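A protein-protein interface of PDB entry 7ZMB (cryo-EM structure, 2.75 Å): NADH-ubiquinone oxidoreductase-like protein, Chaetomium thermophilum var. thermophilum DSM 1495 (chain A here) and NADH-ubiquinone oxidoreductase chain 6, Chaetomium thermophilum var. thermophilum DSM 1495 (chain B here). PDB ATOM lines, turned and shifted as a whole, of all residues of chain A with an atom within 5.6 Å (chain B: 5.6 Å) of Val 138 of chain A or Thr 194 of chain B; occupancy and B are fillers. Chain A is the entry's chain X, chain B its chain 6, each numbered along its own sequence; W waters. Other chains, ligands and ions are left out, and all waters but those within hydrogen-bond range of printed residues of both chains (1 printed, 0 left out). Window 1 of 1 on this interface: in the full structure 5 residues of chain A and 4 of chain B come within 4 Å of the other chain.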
ATOM      1  N   ALA A 134     -11.961  -6.464 -10.854  1.00  0.00           N
ATOM      2  CA  ALA A 134     -13.400  -6.515 -10.517  1.00  0.00           C
ATOM      3  C   ALA A 134     -14.258  -6.614 -11.774  1.00  0.00           C
ATOM      4  O   ALA A 134     -15.266  -7.314 -11.741  1.00  0.00           O
ATOM      5  CB  ALA A 134     -13.788  -5.347  -9.656  1.00  0.00           C
ATOM      6  N   MET A 135     -13.880  -5.905 -12.831  1.00  0.00           N
ATOM      7  CA  MET A 135     -14.642  -5.956 -14.101  1.00  0.00           C
ATOM      8  C   MET A 135     -14.565  -7.370 -14.661  1.00  0.00           C
ATOM      9  O   MET A 135     -15.550  -7.813 -15.251  1.00  0.00           O
ATOM     10  CB  MET A 135     -14.138  -4.926 -15.104  1.00  0.00           C
ATOM     11  CG  MET A 135     -14.988  -3.677 -15.133  1.00  0.00           C
ATOM     12  SD  MET A 135     -16.759  -4.062 -15.183  1.00  0.00           S
ATOM     13  CE  MET A 135     -17.260  -3.546 -13.542  1.00  0.00           C
ATOM     14  N   GLN A 136     -13.429  -8.037 -14.460  1.00  0.00           N
ATOM     15  CA  GLN A 136     -13.237  -9.436 -14.901  1.00  0.00           C
ATOM     16  C   GLN A 136     -14.250 -10.308 -14.184  1.00  0.00           C
ATOM     17  O   GLN A 136     -14.790 -11.203 -14.818  1.00  0.00           O
ATOM     18  CB  GLN A 136     -11.810  -9.882 -14.589  1.00  0.00           C
ATOM     19  CG  GLN A 136     -10.767  -9.230 -15.484  1.00  0.00           C
ATOM     20  CD  GLN A 136      -9.365  -9.508 -15.009  1.00  0.00           C
ATOM     21  OE1 GLN A 136      -8.430  -8.768 -15.303  1.00  0.00           O
ATOM     22  NE2 GLN A 136      -9.213 -10.579 -14.248  1.00  0.00           N
ATOM     23  N   GLY A 137     -14.408 -10.095 -12.880  1.00  0.00           N
ATOM     24  CA  GLY A 137     -15.371 -10.861 -12.078  1.00  0.00           C
ATOM     25  C   GLY A 137     -16.762 -10.714 -12.630  1.00  0.00           C
ATOM     26  O   GLY A 137     -17.441 -11.727 -12.766  1.00  0.00           O
ATOM     27  N   VAL A 138     -17.164  -9.483 -12.927  1.00  0.00           N
ATOM     28  CA  VAL A 138     -18.536  -9.223 -13.448  1.00  0.00           C
ATOM     29  C   VAL A 138     -18.674  -9.978 -14.767  1.00  0.00           C
ATOM     30  O   VAL A 138     -19.720 -10.609 -14.961  1.00  0.00           O
ATOM     31  CB  VAL A 138     -18.787  -7.709 -13.599  1.00  0.00           C
ATOM     32  CG1 VAL A 138     -20.228  -7.407 -13.960  1.00  0.00           C
ATOM     33  CG2 VAL A 138     -18.371  -6.948 -12.354  1.00  0.00           C
ATOM     34  N   ALA A 139     -17.639  -9.958 -15.605  1.00  0.00           N
ATOM     35  CA  ALA A 139     -17.646 -10.684 -16.889  1.00  0.00           C
ATOM     36  C   ALA A 139     -17.746 -12.202 -16.687  1.00  0.00           C
ATOM     37  O   ALA A 139     -18.549 -12.828 -17.390  1.00  0.00           O
ATOM     38  CB  ALA A 139     -16.412 -10.309 -17.664  1.00  0.00           C
ATOM     39  N   ALA A 140     -16.984 -12.765 -15.749  1.00  0.00           N
ATOM     40  CA  ALA A 140     -17.050 -14.215 -15.446  1.00  0.00           C
ATOM     41  C   ALA A 140     -18.442 -14.578 -14.921  1.00  0.00           C
ATOM     42  O   ALA A 140     -18.952 -15.628 -15.307  1.00  0.00           O
ATOM     43  CB  ALA A 140     -15.989 -14.552 -14.433  1.00  0.00           C
ATOM     44  N   ARG A 141     -19.034 -13.725 -14.092  1.00  0.00           N
ATOM     45  CA  ARG A 141     -20.333 -14.027 -13.446  1.00  0.00           C
ATOM     46  C   ARG A 141     -21.487 -13.720 -14.395  1.00  0.00           C
ATOM     47  O   ARG A 141     -22.617 -14.029 -14.046  1.00  0.00           O
ATOM     48  CB  ARG A 141     -20.465 -13.258 -12.129  1.00  0.00           C
ATOM     49  CG  ARG A 141     -19.402 -13.596 -11.095  1.00  0.00           C
ATOM     50  CD  ARG A 141     -19.621 -12.869  -9.785  1.00  0.00           C
ATOM     51  NE  ARG A 141     -19.975 -11.465  -9.931  1.00  0.00           N
ATOM     52  CZ  ARG A 141     -19.158 -10.444  -9.697  1.00  0.00           C
ATOM     53  NH1 ARG A 141     -19.584  -9.205  -9.859  1.00  0.00           N
ATOM     54  NH2 ARG A 141     -17.922 -10.665  -9.293  1.00  0.00           N
ATOM     55  N   GLN A 142     -21.205 -13.143 -15.554  1.00  0.00           N
ATOM     56  CA  GLN A 142     -22.270 -12.883 -16.545  1.00  0.00           C
ATOM     57  C   GLN A 142     -22.247 -14.022 -17.554  1.00  0.00           C
ATOM     58  O   GLN A 142     -23.329 -14.432 -18.005  1.00  0.00           O
ATOM     59  CB  GLN A 142     -22.019 -11.561 -17.260  1.00  0.00           C
ATOM     60  CG  GLN A 142     -22.636 -11.521 -18.647  1.00  0.00           C
ATOM     61  CD  GLN A 142     -23.656 -10.424 -18.787  1.00  0.00           C
ATOM     62  OE1 GLN A 142     -24.843 -10.666 -18.975  1.00  0.00           O
ATOM     63  NE2 GLN A 142     -23.182  -9.196 -18.696  1.00  0.00           N
ATOM     64  N   SER A 143     -21.069 -14.561 -17.840  1.00  0.00           N
ATOM     65  CA  SER A 143     -21.000 -15.579 -18.910  1.00  0.00           C
ATOM     66  C   SER A 143     -20.763 -17.032 -18.496  1.00  0.00           C
ATOM     67  O   SER A 143     -20.821 -17.872 -19.384  1.00  0.00           O
ATOM     68  CB  SER A 143     -19.989 -15.130 -19.914  1.00  0.00           C
ATOM     69  OG  SER A 143     -18.798 -14.690 -19.291  1.00  0.00           O
ATOM     70  N   ASN B 190     -22.023   2.995 -12.413  1.00  0.00           N
ATOM     71  CA  ASN B 190     -20.963   2.033 -12.138  1.00  0.00           C
ATOM     72  C   ASN B 190     -21.439   0.594 -12.257  1.00  0.00           C
ATOM     73  O   ASN B 190     -20.610  -0.307 -12.401  1.00  0.00           O
ATOM     74  CB  ASN B 190     -20.387   2.271 -10.744  1.00  0.00           C
ATOM     75  CG  ASN B 190     -19.443   3.458 -10.691  1.00  0.00           C
ATOM     76  OD1 ASN B 190     -18.957   3.930 -11.714  1.00  0.00           O
ATOM     77  ND2 ASN B 190     -19.185   3.949  -9.487  1.00  0.00           N
ATOM     78  N   ILE B 191     -22.747   0.353 -12.193  1.00  0.00           N
ATOM     79  CA  ILE B 191     -23.281  -1.006 -12.185  1.00  0.00           C
ATOM     80  C   ILE B 191     -24.441  -1.215 -13.144  1.00  0.00           C
ATOM     81  O   ILE B 191     -24.796  -2.370 -13.432  1.00  0.00           O
ATOM     82  CB  ILE B 191     -23.697  -1.403 -10.752  1.00  0.00           C
ATOM     83  CG1 ILE B 191     -24.796  -0.469 -10.268  1.00  0.00           C
ATOM     84  CG2 ILE B 191     -22.516  -1.383  -9.805  1.00  0.00           C
ATOM     85  CD1 ILE B 191     -25.403  -0.901  -9.024  1.00  0.00           C
ATOM     86  N   MET B 192     -25.066  -0.167 -13.674  1.00  0.00           N
ATOM     87  CA  MET B 192     -26.227  -0.329 -14.540  1.00  0.00           C
ATOM     88  C   MET B 192     -25.874  -1.000 -15.866  1.00  0.00           C
ATOM     89  O   MET B 192     -26.754  -1.567 -16.520  1.00  0.00           O
ATOM     90  CB  MET B 192     -26.870   1.052 -14.747  1.00  0.00           C
ATOM     91  CG  MET B 192     -27.772   1.216 -15.947  1.00  0.00           C
ATOM     92  SD  MET B 192     -28.503   2.856 -16.030  1.00  0.00           S
ATOM     93  CE  MET B 192     -29.987   2.608 -15.062  1.00  0.00           C
ATOM     94  N   TYR B 193     -24.602  -0.981 -16.256  1.00  0.00           N
ATOM     95  CA  TYR B 193     -24.174  -1.501 -17.543  1.00  0.00           C
ATOM     96  C   TYR B 193     -23.218  -2.680 -17.448  1.00  0.00           C
ATOM     97  O   TYR B 193     -22.810  -3.209 -18.484  1.00  0.00           O
ATOM     98  CB  TYR B 193     -23.526  -0.384 -18.375  1.00  0.00           C
ATOM     99  CG  TYR B 193     -24.351   0.866 -18.463  1.00  0.00           C
ATOM    100  CD1 TYR B 193     -25.312   1.013 -19.443  1.00  0.00           C
ATOM    101  CD2 TYR B 193     -24.182   1.892 -17.557  1.00  0.00           C
ATOM    102  CE1 TYR B 193     -26.073   2.148 -19.522  1.00  0.00           C
ATOM    103  CE2 TYR B 193     -24.937   3.028 -17.626  1.00  0.00           C
ATOM    104  CZ  TYR B 193     -25.880   3.155 -18.615  1.00  0.00           C
ATOM    105  OH  TYR B 193     -26.627   4.298 -18.681  1.00  0.00           O
ATOM    106  N   THR B 194     -22.981  -3.190 -16.252  1.00  0.00           N
ATOM    107  CA  THR B 194     -22.146  -4.407 -16.117  1.00  0.00           C
ATOM    108  C   THR B 194     -22.870  -5.398 -15.214  1.00  0.00           C
ATOM    109  O   THR B 194     -23.393  -6.374 -15.751  1.00  0.00           O
ATOM    110  CB  THR B 194     -20.748  -4.073 -15.581  1.00  0.00           C
ATOM    111  OG1 THR B 194     -20.863  -3.360 -14.349  1.00  0.00           O
ATOM    112  CG2 THR B 194     -19.913  -3.276 -16.560  1.00  0.00           C
ATOM    113  N   ASN B 195     -22.933  -5.123 -13.915  1.00  0.00           N
ATOM    114  CA  ASN B 195     -23.501  -6.068 -12.916  1.00  0.00           C
ATOM    115  C   ASN B 195     -24.984  -6.349 -13.167  1.00  0.00           C
ATOM    116  O   ASN B 195     -25.396  -7.496 -12.958  1.00  0.00           O
ATOM    117  CB  ASN B 195     -23.252  -5.527 -11.508  1.00  0.00           C
ATOM    118  CG  ASN B 195     -21.801  -5.208 -11.220  1.00  0.00           C
ATOM    119  OD1 ASN B 195     -21.304  -4.150 -11.591  1.00  0.00           O
ATOM    120  ND2 ASN B 195     -21.114  -6.113 -10.543  1.00  0.00           N
ATOM    121  N   TYR B 196     -25.760  -5.341 -13.572  1.00  0.00           N
ATOM    122  CA  TYR B 196     -27.228  -5.516 -13.736  1.00  0.00           C
ATOM    123  C   TYR B 196     -27.659  -5.260 -15.189  1.00  0.00           C
ATOM    124  O   TYR B 196     -28.815  -4.887 -15.390  1.00  0.00           O
ATOM    125  CB  TYR B 196     -27.953  -4.691 -12.670  1.00  0.00           C
ATOM    126  CG  TYR B 196     -27.516  -5.021 -11.265  1.00  0.00           C
ATOM    127  CD1 TYR B 196     -28.075  -6.081 -10.573  1.00  0.00           C
ATOM    128  CD2 TYR B 196     -26.512  -4.300 -10.643  1.00  0.00           C
ATOM    129  CE1 TYR B 196     -27.665  -6.402  -9.291  1.00  0.00           C
ATOM    130  CE2 TYR B 196     -26.079  -4.618  -9.368  1.00  0.00           C
ATOM    131  CZ  TYR B 196     -26.661  -5.669  -8.685  1.00  0.00           C
ATOM    132  OH  TYR B 196     -26.245  -5.973  -7.422  1.00  0.00           O
ATOM    133  N   ASN B 197     -26.795  -5.529 -16.164  1.00  0.00           N
ATOM    134  CA  ASN B 197     -27.104  -5.267 -17.597  1.00  0.00           C
ATOM    135  C   ASN B 197     -28.300  -6.084 -18.128  1.00  0.00           C
ATOM    136  O   ASN B 197     -28.817  -5.707 -19.182  1.00  0.00           O
ATOM    137  CB  ASN B 197     -25.836  -5.220 -18.464  1.00  0.00           C
ATOM    138  CG  ASN B 197     -25.116  -6.533 -18.653  1.00  0.00           C
ATOM    139  OD1 ASN B 197     -25.700  -7.605 -18.524  1.00  0.00           O
ATOM    140  ND2 ASN B 197     -23.844  -6.449 -18.996  1.00  0.00           N
HETATM  141  O   HOH W   1     -23.827  -8.856 -16.078  1.00  0.00           O
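NE2 of Gln 142 of chain A sits close to ND2 of Asn 197 of chain B, at 2.8 Å.
The side-chain amide nitrogen of Asn 197 of chain B sits at hydrogen-bond distance from the backbone carbonyl oxygen of Tyr 193 of chain B (3.4 Å).
The side-chain amide oxygen (OD1) of Asn 195 of chain B lies within hydrogen-bond range of the side-chain hydroxyl (OG1) of Thr 194 of chain B (2.9 Å).
ND2 of Asn 197 of chain B lies within hydrogen-bond range of O of Thr 194 of chain B (3.3 Å).
Among the printed residues, merely in contact across the chains: Val 138 of chain A with Asn 195 of chain B, Arg 141 of chain A with Asn 195 of chain B, Met 135 of chain A with Thr 194 of chain B and Val 138 of chain A with Thr 194 of chain B.
Printed residues of chain B within 4 Å of Met 135 of chain A: Thr 194.
Val 138 of chain A touches two residues of chain B.
Printed residues of chain B within 4 Å of Arg 141 of chain A: Asn 195.
Of the printed residues of chain B, Gln 142 of chain A touches Asn 197.
Tyr 193 of chain B touches none of the printed residues of chain A.
Of the printed residues of chain A, Thr 194 of chain B touches Met 135 (3.5 Å) and Val 138 (3.5 Å).
Printed residues of chain A within 4 Å of Asn 195 of chain B: Val 138 and Arg 141.
Tyr 196 of chain B touches none of the printed residues of chain A.
Printed residues of chain A within 4 Å of Asn 197 of chain B: Gln 142.
The nearest printed residue of chain B that does not touch Val 138 of chain A is Tyr 196 of chain B (5.9 Å).
The nearest residue of chain A that does not touch Thr 194 of chain B is Gln 142 of chain A (4.1 Å).
Of the 10 printed residues of chain A, 4 touch a printed residue of chain B.
Hydrophobic or aromatic side chains of chain A within 4 Å of the printed part of chain B: Met 135 and Val 138.
Printed residues of chain B that touch a printed residue of chain A: Thr 194, Asn 195 and Asn 197.
Among the printed residues, no Asp or Glu carboxylate lies within 4 Å of a Lys or Arg side-chain nitrogen of the other chain.
Water W1 lies within hydrogen-bond range of the backbone carbonyl oxygen (O) of Thr 194 of chain B (2.5 Å), the side-chain amide nitrogen (NE2) of Gln 142 of chain A (2.7 Å) and the side-chain amide oxygen (OD1) of Asn 197 of chain B (3.3 Å).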
